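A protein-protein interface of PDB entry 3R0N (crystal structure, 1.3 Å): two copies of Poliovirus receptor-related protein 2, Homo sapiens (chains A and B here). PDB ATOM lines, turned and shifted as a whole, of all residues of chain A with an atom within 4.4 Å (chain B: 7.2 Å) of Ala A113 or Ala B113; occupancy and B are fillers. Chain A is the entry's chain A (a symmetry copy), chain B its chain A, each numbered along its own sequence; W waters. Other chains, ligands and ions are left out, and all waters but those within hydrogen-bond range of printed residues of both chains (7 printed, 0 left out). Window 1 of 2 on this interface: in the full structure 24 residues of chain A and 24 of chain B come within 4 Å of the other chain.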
ATOM      1  N   TYR A  34      -2.738  28.784  14.108  1.00  0.00           N
ATOM      2  CA  TYR A  34      -1.746  27.840  14.586  1.00  0.00           C
ATOM      3  C   TYR A  34      -0.435  28.041  13.832  1.00  0.00           C
ATOM      4  O   TYR A  34      -0.412  27.997  12.593  1.00  0.00           O
ATOM      5  CB  TYR A  34      -2.239  26.399  14.394  1.00  0.00           C
ATOM      6  CG  TYR A  34      -1.325  25.395  15.065  1.00  0.00           C
ATOM      7  CD1 TYR A  34      -1.359  25.230  16.446  1.00  0.00           C
ATOM      8  CD2 TYR A  34      -0.410  24.633  14.333  1.00  0.00           C
ATOM      9  CE1 TYR A  34      -0.528  24.357  17.089  1.00  0.00           C
ATOM     10  CE2 TYR A  34       0.435  23.723  14.967  1.00  0.00           C
ATOM     11  CZ  TYR A  34       0.359  23.599  16.354  1.00  0.00           C
ATOM     12  OH  TYR A  34       1.153  22.722  17.050  1.00  0.00           O
ATOM     13  N   ILE A  35       0.656  28.218  14.577  1.00  0.00           N
ATOM     14  CA  ILE A  35       1.979  28.297  13.954  1.00  0.00           C
ATOM     15  C   ILE A  35       2.591  26.904  13.942  1.00  0.00           C
ATOM     16  O   ILE A  35       2.985  26.375  14.991  1.00  0.00           O
ATOM     17  CB  ILE A  35       2.906  29.298  14.654  1.00  0.00           C
ATOM     18  CG1 ILE A  35       2.262  30.699  14.732  1.00  0.00           C
ATOM     19  CG2 ILE A  35       4.239  29.318  13.911  1.00  0.00           C
ATOM     20  CD1 ILE A  35       3.056  31.703  15.543  1.00  0.00           C
ATOM     21  N   SER A  36       2.629  26.302  12.758  1.00  0.00           N
ATOM     22  CA  SER A  36       3.144  24.939  12.589  1.00  0.00           C
ATOM     23  C   SER A  36       4.671  24.866  12.583  1.00  0.00           C
ATOM     24  O   SER A  36       5.248  23.865  13.004  1.00  0.00           O
ATOM     25  CB  SER A  36       2.590  24.314  11.307  1.00  0.00           C
ATOM     26  OG  SER A  36       1.236  23.934  11.453  1.00  0.00           O
ATOM     27  N   LEU A  37       5.325  25.907  12.086  1.00  0.00           N
ATOM     28  CA  LEU A  37       6.778  25.887  11.938  1.00  0.00           C
ATOM     29  C   LEU A  37       7.246  27.299  11.684  1.00  0.00           C
ATOM     30  O   LEU A  37       6.503  28.100  11.099  1.00  0.00           O
ATOM     31  CB  LEU A  37       7.188  25.014  10.731  1.00  0.00           C
ATOM     32  CG  LEU A  37       8.615  24.478  10.724  1.00  0.00           C
ATOM     33  CD1 LEU A  37       8.745  23.306  11.707  1.00  0.00           C
ATOM     34  CD2 LEU A  37       9.020  24.015   9.336  1.00  0.00           C
ATOM     35  N   GLU A 111      10.265  32.889   7.887  1.00  0.00           N
ATOM     36  CA  GLU A 111       9.008  32.378   7.347  1.00  0.00           C
ATOM     37  C   GLU A 111       8.219  31.606   8.382  1.00  0.00           C
ATOM     38  O   GLU A 111       8.752  30.709   9.022  1.00  0.00           O
ATOM     39  CB  GLU A 111       9.304  31.482   6.140  1.00  0.00           C
ATOM     40  CG  GLU A 111       8.099  30.968   5.344  1.00  0.00           C
ATOM     41  CD  GLU A 111       8.559  30.531   3.948  1.00  0.00           C
ATOM     42  OE1 GLU A 111       8.862  29.335   3.779  1.00  0.00           O
ATOM     43  OE2 GLU A 111       8.711  31.398   3.042  1.00  0.00           O
ATOM     44  N   PHE A 112       6.948  31.950   8.517  1.00  0.00           N
ATOM     45  CA  PHE A 112       6.031  31.215   9.383  1.00  0.00           C
ATOM     46  C   PHE A 112       5.104  30.376   8.533  1.00  0.00           C
ATOM     47  O   PHE A 112       4.450  30.895   7.610  1.00  0.00           O
ATOM     48  CB  PHE A 112       5.148  32.172  10.199  1.00  0.00           C
ATOM     49  CG  PHE A 112       5.895  32.965  11.215  1.00  0.00           C
ATOM     50  CD1 PHE A 112       5.916  32.564  12.543  1.00  0.00           C
ATOM     51  CD2 PHE A 112       6.570  34.125  10.849  1.00  0.00           C
ATOM     52  CE1 PHE A 112       6.598  33.321  13.485  1.00  0.00           C
ATOM     53  CE2 PHE A 112       7.238  34.874  11.792  1.00  0.00           C
ATOM     54  CZ  PHE A 112       7.260  34.468  13.104  1.00  0.00           C
ATOM     55  N   ALA A 113       5.026  29.092   8.857  1.00  0.00           N
ATOM     56  CA  ALA A 113       4.076  28.160   8.233  1.00  0.00           C
ATOM     57  C   ALA A 113       2.878  28.062   9.182  1.00  0.00           C
ATOM     58  O   ALA A 113       2.997  27.519  10.282  1.00  0.00           O
ATOM     59  CB  ALA A 113       4.730  26.818   8.005  1.00  0.00           C
ATOM     60  N   THR A 114       1.751  28.651   8.792  1.00  0.00           N
ATOM     61  CA  THR A 114       0.597  28.790   9.672  1.00  0.00           C
ATOM     62  C   THR A 114      -0.631  28.105   9.114  1.00  0.00           C
ATOM     63  O   THR A 114      -0.770  27.938   7.894  1.00  0.00           O
ATOM     64  CB  THR A 114       0.230  30.276   9.953  1.00  0.00           C
ATOM     65  OG1 THR A 114      -0.538  30.833   8.874  1.00  0.00           O
ATOM     66  CG2 THR A 114       1.464  31.090  10.247  1.00  0.00           C
ATOM     67  N   GLY A 118      -1.614  29.812   5.902  1.00  0.00           N
ATOM     68  CA  GLY A 118      -0.509  29.423   5.054  1.00  0.00           C
ATOM     69  C   GLY A 118       0.815  30.052   5.432  1.00  0.00           C
ATOM     70  O   GLY A 118       1.036  30.445   6.586  1.00  0.00           O
ATOM     71  N   SER A 119       1.724  30.126   4.475  1.00  0.00           N
ATOM     72  CA  SER A 119       3.093  30.539   4.798  1.00  0.00           C
ATOM     73  C   SER A 119       3.361  31.958   4.368  1.00  0.00           C
ATOM     74  O   SER A 119       3.064  32.360   3.245  1.00  0.00           O
ATOM     75  CB  SER A 119       4.120  29.598   4.198  1.00  0.00           C
ATOM     76  OG  SER A 119       3.945  28.346   4.792  1.00  0.00           O
ATOM     77  N   LEU B  26       6.935  15.137  -2.055  1.00  0.00           N
ATOM     78  CA  LEU B  26       8.188  15.346  -1.316  1.00  0.00           C
ATOM     79  C   LEU B  26       9.051  14.091  -1.406  1.00  0.00           C
ATOM     80  O   LEU B  26       8.615  13.020  -0.977  1.00  0.00           O
ATOM     81  CB  LEU B  26       7.889  15.693   0.156  1.00  0.00           C
ATOM     82  CG  LEU B  26       9.095  16.141   0.979  1.00  0.00           C
ATOM     83  CD1 LEU B  26       9.617  17.513   0.515  1.00  0.00           C
ATOM     84  CD2 LEU B  26       8.744  16.197   2.462  1.00  0.00           C
ATOM     85  N   TYR B  34       9.384  15.065   9.671  1.00  0.00           N
ATOM     86  CA  TYR B  34       8.011  15.418   9.976  1.00  0.00           C
ATOM     87  C   TYR B  34       7.532  16.506   9.018  1.00  0.00           C
ATOM     88  O   TYR B  34       8.166  17.567   8.909  1.00  0.00           O
ATOM     89  CB  TYR B  34       7.892  15.913  11.424  1.00  0.00           C
ATOM     90  CG  TYR B  34       6.448  16.097  11.842  1.00  0.00           C
ATOM     91  CD1 TYR B  34       5.662  14.991  12.148  1.00  0.00           C
ATOM     92  CD2 TYR B  34       5.858  17.362  11.905  1.00  0.00           C
ATOM     93  CE1 TYR B  34       4.347  15.116  12.499  1.00  0.00           C
ATOM     94  CE2 TYR B  34       4.524  17.513  12.279  1.00  0.00           C
ATOM     95  CZ  TYR B  34       3.781  16.371  12.574  1.00  0.00           C
ATOM     96  OH  TYR B  34       2.464  16.437  12.953  1.00  0.00           O
ATOM     97  N   ILE B  35       6.397  16.262   8.363  1.00  0.00           N
ATOM     98  CA  ILE B  35       5.790  17.290   7.516  1.00  0.00           C
ATOM     99  C   ILE B  35       4.779  18.066   8.348  1.00  0.00           C
ATOM    100  O   ILE B  35       3.708  17.547   8.691  1.00  0.00           O
ATOM    101  CB  ILE B  35       5.135  16.711   6.256  1.00  0.00           C
ATOM    102  CG1 ILE B  35       6.138  15.865   5.442  1.00  0.00           C
ATOM    103  CG2 ILE B  35       4.561  17.866   5.440  1.00  0.00           C
ATOM    104  CD1 ILE B  35       5.522  15.138   4.264  1.00  0.00           C
ATOM    105  N   SER B  36       5.145  19.294   8.702  1.00  0.00           N
ATOM    106  CA  SER B  36       4.302  20.149   9.544  1.00  0.00           C
ATOM    107  C   SER B  36       3.149  20.802   8.781  1.00  0.00           C
ATOM    108  O   SER B  36       2.090  21.056   9.352  1.00  0.00           O
ATOM    109  CB  SER B  36       5.148  21.226  10.226  1.00  0.00           C
ATOM    110  OG  SER B  36       5.914  20.696  11.290  1.00  0.00           O
ATOM    111  N   LEU B  37       3.358  21.096   7.505  1.00  0.00           N
ATOM    112  CA  LEU B  37       2.358  21.818   6.722  1.00  0.00           C
ATOM    113  C   LEU B  37       2.724  21.696   5.263  1.00  0.00           C
ATOM    114  O   LEU B  37       3.913  21.586   4.931  1.00  0.00           O
ATOM    115  CB  LEU B  37       2.352  23.316   7.099  1.00  0.00           C
ATOM    116  CG  LEU B  37       1.086  24.101   6.776  1.00  0.00           C
ATOM    117  CD1 LEU B  37      -0.017  23.767   7.791  1.00  0.00           C
ATOM    118  CD2 LEU B  37       1.347  25.596   6.794  1.00  0.00           C
ATOM    119  N   VAL B  38       1.721  21.746   4.391  1.00  0.00           N
ATOM    120  CA  VAL B  38       1.967  22.004   2.984  1.00  0.00           C
ATOM    121  C   VAL B  38       1.121  23.193   2.578  1.00  0.00           C
ATOM    122  O   VAL B  38      -0.008  23.372   3.059  1.00  0.00           O
ATOM    123  CB  VAL B  38       1.651  20.800   2.076  1.00  0.00           C
ATOM    124  CG1 VAL B  38       2.452  19.625   2.475  1.00  0.00           C
ATOM    125  CG2 VAL B  38       0.206  20.468   2.108  1.00  0.00           C
ATOM    126  N   THR B  39       1.683  24.015   1.698  1.00  0.00           N
ATOM    127  CA  THR B  39       0.948  25.138   1.125  1.00  0.00           C
ATOM    128  C   THR B  39       1.090  25.189  -0.383  1.00  0.00           C
ATOM    129  O   THR B  39       2.096  24.727  -0.940  1.00  0.00           O
ATOM    130  CB  THR B  39       1.364  26.499   1.725  1.00  0.00           C
ATOM    131  OG1 THR B  39       2.729  26.772   1.420  1.00  0.00           O
ATOM    132  CG2 THR B  39       1.132  26.548   3.206  1.00  0.00           C
ATOM    133  N   HIS B  56      -2.906  20.963   6.974  1.00  0.00           N
ATOM    134  CA  HIS B  56      -2.336  20.660   8.278  1.00  0.00           C
ATOM    135  C   HIS B  56      -2.614  19.179   8.605  1.00  0.00           C
ATOM    136  O   HIS B  56      -3.714  18.685   8.345  1.00  0.00           O
ATOM    137  CB  HIS B  56      -2.985  21.582   9.319  1.00  0.00           C
ATOM    138  CG  HIS B  56      -2.436  21.450  10.694  1.00  0.00           C
ATOM    139  ND1 HIS B  56      -2.840  20.459  11.567  1.00  0.00           N
ATOM    140  CD2 HIS B  56      -1.534  22.208  11.360  1.00  0.00           C
ATOM    141  CE1 HIS B  56      -2.170  20.594  12.700  1.00  0.00           C
ATOM    142  NE2 HIS B  56      -1.398  21.664  12.612  1.00  0.00           N
ATOM    143  N   LEU B  90       0.855  13.704   4.177  1.00  0.00           N
ATOM    144  CA  LEU B  90       1.000  14.924   3.400  1.00  0.00           C
ATOM    145  C   LEU B  90       2.026  14.807   2.283  1.00  0.00           C
ATOM    146  O   LEU B  90       2.196  15.748   1.532  1.00  0.00           O
ATOM    147  CB  LEU B  90       1.362  16.101   4.316  1.00  0.00           C
ATOM    148  CG  LEU B  90       0.210  16.827   5.014  1.00  0.00           C
ATOM    149  CD1 LEU B  90      -0.598  15.894   5.916  1.00  0.00           C
ATOM    150  CD2 LEU B  90       0.752  17.998   5.788  1.00  0.00           C
ATOM    151  N   GLU B 111       4.817  24.020  -1.445  1.00  0.00           N
ATOM    152  CA  GLU B 111       5.827  24.151  -0.399  1.00  0.00           C
ATOM    153  C   GLU B 111       5.537  23.252   0.783  1.00  0.00           C
ATOM    154  O   GLU B 111       4.435  23.266   1.314  1.00  0.00           O
ATOM    155  CB  GLU B 111       5.896  25.610   0.059  1.00  0.00           C
ATOM    156  CG  GLU B 111       7.006  25.977   1.051  1.00  0.00           C
ATOM    157  CD  GLU B 111       7.242  27.491   1.017  1.00  0.00           C
ATOM    158  OE1 GLU B 111       6.624  28.199   1.834  1.00  0.00           O
ATOM    159  OE2 GLU B 111       7.970  27.988   0.112  1.00  0.00           O
ATOM    160  N   PHE B 112       6.542  22.495   1.197  1.00  0.00           N
ATOM    161  CA  PHE B 112       6.452  21.672   2.398  1.00  0.00           C
ATOM    162  C   PHE B 112       7.254  22.316   3.507  1.00  0.00           C
ATOM    163  O   PHE B 112       8.445  22.629   3.326  1.00  0.00           O
ATOM    164  CB  PHE B 112       7.052  20.277   2.164  1.00  0.00           C
ATOM    165  CG  PHE B 112       6.276  19.438   1.209  1.00  0.00           C
ATOM    166  CD1 PHE B 112       5.381  18.486   1.677  1.00  0.00           C
ATOM    167  CD2 PHE B 112       6.447  19.587  -0.163  1.00  0.00           C
ATOM    168  CE1 PHE B 112       4.678  17.696   0.779  1.00  0.00           C
ATOM    169  CE2 PHE B 112       5.749  18.793  -1.047  1.00  0.00           C
ATOM    170  CZ  PHE B 112       4.861  17.858  -0.578  1.00  0.00           C
ATOM    171  N   ALA B 113       6.615  22.490   4.656  1.00  0.00           N
ATOM    172  CA  ALA B 113       7.273  22.971   5.879  1.00  0.00           C
ATOM    173  C   ALA B 113       7.605  21.728   6.710  1.00  0.00           C
ATOM    174  O   ALA B 113       6.703  21.059   7.219  1.00  0.00           O
ATOM    175  CB  ALA B 113       6.369  23.924   6.623  1.00  0.00           C
ATOM    176  N   THR B 114       8.886  21.378   6.784  1.00  0.00           N
ATOM    177  CA  THR B 114       9.319  20.122   7.385  1.00  0.00           C
ATOM    178  C   THR B 114      10.248  20.343   8.559  1.00  0.00           C
ATOM    179  O   THR B 114      10.940  21.367   8.642  1.00  0.00           O
ATOM    180  CB  THR B 114      10.042  19.187   6.373  1.00  0.00           C
ATOM    181  OG1 THR B 114      11.416  19.569   6.205  1.00  0.00           O
ATOM    182  CG2 THR B 114       9.303  19.141   5.060  1.00  0.00           C
ATOM    183  N   PHE B 115      10.305  19.343   9.437  1.00  0.00           N
ATOM    184  CA  PHE B 115      11.270  19.358  10.530  1.00  0.00           C
ATOM    185  C   PHE B 115      12.017  18.034  10.485  1.00  0.00           C
ATOM    186  O   PHE B 115      11.379  17.002  10.455  1.00  0.00           O
ATOM    187  CB  PHE B 115      10.588  19.558  11.886  1.00  0.00           C
ATOM    188  CG  PHE B 115      11.572  19.797  12.991  1.00  0.00           C
ATOM    189  CD1 PHE B 115      12.097  21.068  13.184  1.00  0.00           C
ATOM    190  CD2 PHE B 115      12.063  18.747  13.759  1.00  0.00           C
ATOM    191  CE1 PHE B 115      13.065  21.308  14.173  1.00  0.00           C
ATOM    192  CE2 PHE B 115      13.011  18.983  14.761  1.00  0.00           C
ATOM    193  CZ  PHE B 115      13.518  20.271  14.958  1.00  0.00           C
ATOM    194  N   LYS B 117      14.336  19.600   8.416  1.00  0.00           N
ATOM    195  CA  LYS B 117      14.985  20.139   7.208  1.00  0.00           C
ATOM    196  C   LYS B 117      14.547  21.545   6.818  1.00  0.00           C
ATOM    197  O   LYS B 117      15.240  22.220   6.052  1.00  0.00           O
ATOM    198  CB  LYS B 117      14.790  19.175   6.033  1.00  0.00           C
ATOM    199  CG  LYS B 117      15.567  17.862   6.165  1.00  0.00           C
ATOM    200  CD  LYS B 117      17.074  18.021   5.969  1.00  0.00           C
ATOM    201  CE  LYS B 117      17.788  16.706   6.126  1.00  0.00           C
ATOM    202  NZ  LYS B 117      19.207  16.788   5.708  1.00  0.00           N
ATOM    203  N   GLY B 118      13.398  21.992   7.316  1.00  0.00           N
ATOM    204  CA  GLY B 118      12.883  23.294   6.953  1.00  0.00           C
ATOM    205  C   GLY B 118      11.958  23.283   5.754  1.00  0.00           C
ATOM    206  O   GLY B 118      11.332  22.264   5.433  1.00  0.00           O
ATOM    207  N   SER B 119      11.833  24.424   5.098  1.00  0.00           N
ATOM    208  CA  SER B 119      10.818  24.557   4.050  1.00  0.00           C
ATOM    209  C   SER B 119      11.428  24.499   2.674  1.00  0.00           C
ATOM    210  O   SER B 119      12.416  25.167   2.377  1.00  0.00           O
ATOM    211  CB  SER B 119      10.001  25.825   4.217  1.00  0.00           C
ATOM    212  OG  SER B 119       9.301  25.722   5.421  1.00  0.00           O
ATOM    213  N   VAL B 120      10.839  23.646   1.852  1.00  0.00           N
ATOM    214  CA  VAL B 120      11.315  23.414   0.491  1.00  0.00           C
ATOM    215  C   VAL B 120      10.147  23.536  -0.478  1.00  0.00           C
ATOM    216  O   VAL B 120       8.990  23.280  -0.103  1.00  0.00           O
ATOM    217  CB  VAL B 120      12.033  22.048   0.333  1.00  0.00           C
ATOM    218  CG1 VAL B 120      13.359  22.080   1.108  1.00  0.00           C
ATOM    219  CG2 VAL B 120      11.166  20.873   0.797  1.00  0.00           C
HETATM  220  O   HOH W   1      -0.404  20.183  15.410  1.00  0.00           O
HETATM  221  O   HOH W   2       4.108  25.330   3.540  1.00  0.00           O
HETATM  222  O   HOH W   3       6.444  26.387   4.023  1.00  0.00           O
HETATM  223  O   HOH W   4       1.757  21.140  12.040  1.00  0.00           O
HETATM  224  O   HOH W   5       7.077  28.106   5.626  1.00  0.00           O
HETATM  225  O   HOH W   6       4.078  21.453  13.405  1.00  0.00           O
HETATM  226  O   HOH W   7       8.630  27.952   7.716  1.00  0.00           O
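The backbone carbonyl oxygen (O) of Thr B39 lies within hydrogen-bond range of the backbone NH (N) of Glu B111 (2.9 Å). The side-chain hydroxyl (OG1) of Thr B114 lies within hydrogen-bond range of the backbone carbonyl oxygen (O) of Gly B118, at 2.8 Å. The backbone carbonyl oxygen (O) of Gly A118 sits at hydrogen-bond distance from the side-chain hydroxyl (OG1) of Thr A114 (2.8 Å). The backbone NH (N) of Ala A113 is in hydrogen-bond range of the backbone carbonyl oxygen (O) of Leu A37, 2.9 Å away. The backbone NH of Ala B113 is in hydrogen-bond range of the backbone carbonyl oxygen of Leu B37 (2.9 Å). The backbone carbonyl oxygen (O) of Ala A113 sits at hydrogen-bond distance from the backbone NH (N) of Ser A36, 2.8 Å away.
Water W4 lies within hydrogen-bond range of O of Ser B36, OG of Ser A36 and NE2 of His B56. Water W6 bridges the backbone carbonyl oxygen (O) of Ser A36 (2.7 Å) and the side-chain hydroxyl (OG) of Ser B36 (2.9 Å). Water W3 lies within hydrogen-bond range of OE1 of Glu B111 (2.8 Å), OG of Ser B119 (3.2 Å) and OG of Ser A119 (3.3 Å). Water W2 lies within hydrogen-bond range of OG1 of Thr B39 (2.9 Å), O of Glu B111 (3.1 Å) and OG of Ser A119 (3.3 Å). Water W7 bridges the backbone carbonyl oxygen (O) of Glu A111 and the side-chain hydroxyl (OG) of Ser B119. Water W1 bridges a ring nitrogen (NE2) of His B56 and the side-chain hydroxyl (OH) of Tyr A34.
Ser A36 touches its own counterpart, Ser B36. Leu A37 touches Ala B113, and with the chains exchanged Ala A113 touches Leu B37. Leu A37 touches Thr B114, and with the chains exchanged Thr A114 touches Leu B37. Ala A113 touches its own counterpart, Ala B113.
Printed residues of chain B within 4 Å of Leu A37: Ser B36, Ala B113 and Thr B114. Ala A113 touches just these residues of chain B: Leu B37 and Ala B113. Of the printed residues of chain B, Thr A114 touches Leu B37 (3.3 Å). Leu B26 touches none of the printed residues of chain A. Of the printed residues of chain A, Leu B37 touches Ser A36 (3.9 Å), Ala A113 (3.8 Å) and Thr A114 (3.3 Å). Ala B113 touches just these residues of chain A: Leu A37 and Ala A113. Of the printed residues of chain A, Thr B114 touches Leu A37 (3.3 Å). The nearest printed residue of chain A that does not touch Ala B113 is Ser A119 (5.4 Å).
The side-chain carboxylate (OE1) of Glu A111 lies close to the side-chain carboxylate (OE1) of Glu B111 (3.2 Å).
Printed residues of chain A that touch a printed residue of chain B: Tyr A34, Ser A36, Leu A37, Glu A111, Ala A113, Thr A114, Gly A118 and Ser A119. Among the printed residues, no Asp or Glu carboxylate lies within 4 Å of a Lys or Arg side-chain nitrogen of the other chain.
Tyr A34 touches His B56 (CD2 to NE2, 3.6 Å). O of Ser A36 touches OG of Ser B36 (3.7 Å). Ser A36 touches Leu B37 (OG to CD1, 3.9 Å). Leu A37 touches Ala B113. Glu A111 touches Ser B119 (OE1 to CB, 3.7 Å). Ala A113 touches Leu B37 (C to CD2, 3.8 Å). Thr A114 touches Leu B37. Thr B39 touches Gly A118 (CG2 to CA, 3.8 Å). Thr B39 touches Ser A119 (CG2 to OG, 3.7 Å). Glu B111 touches Ser A119.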
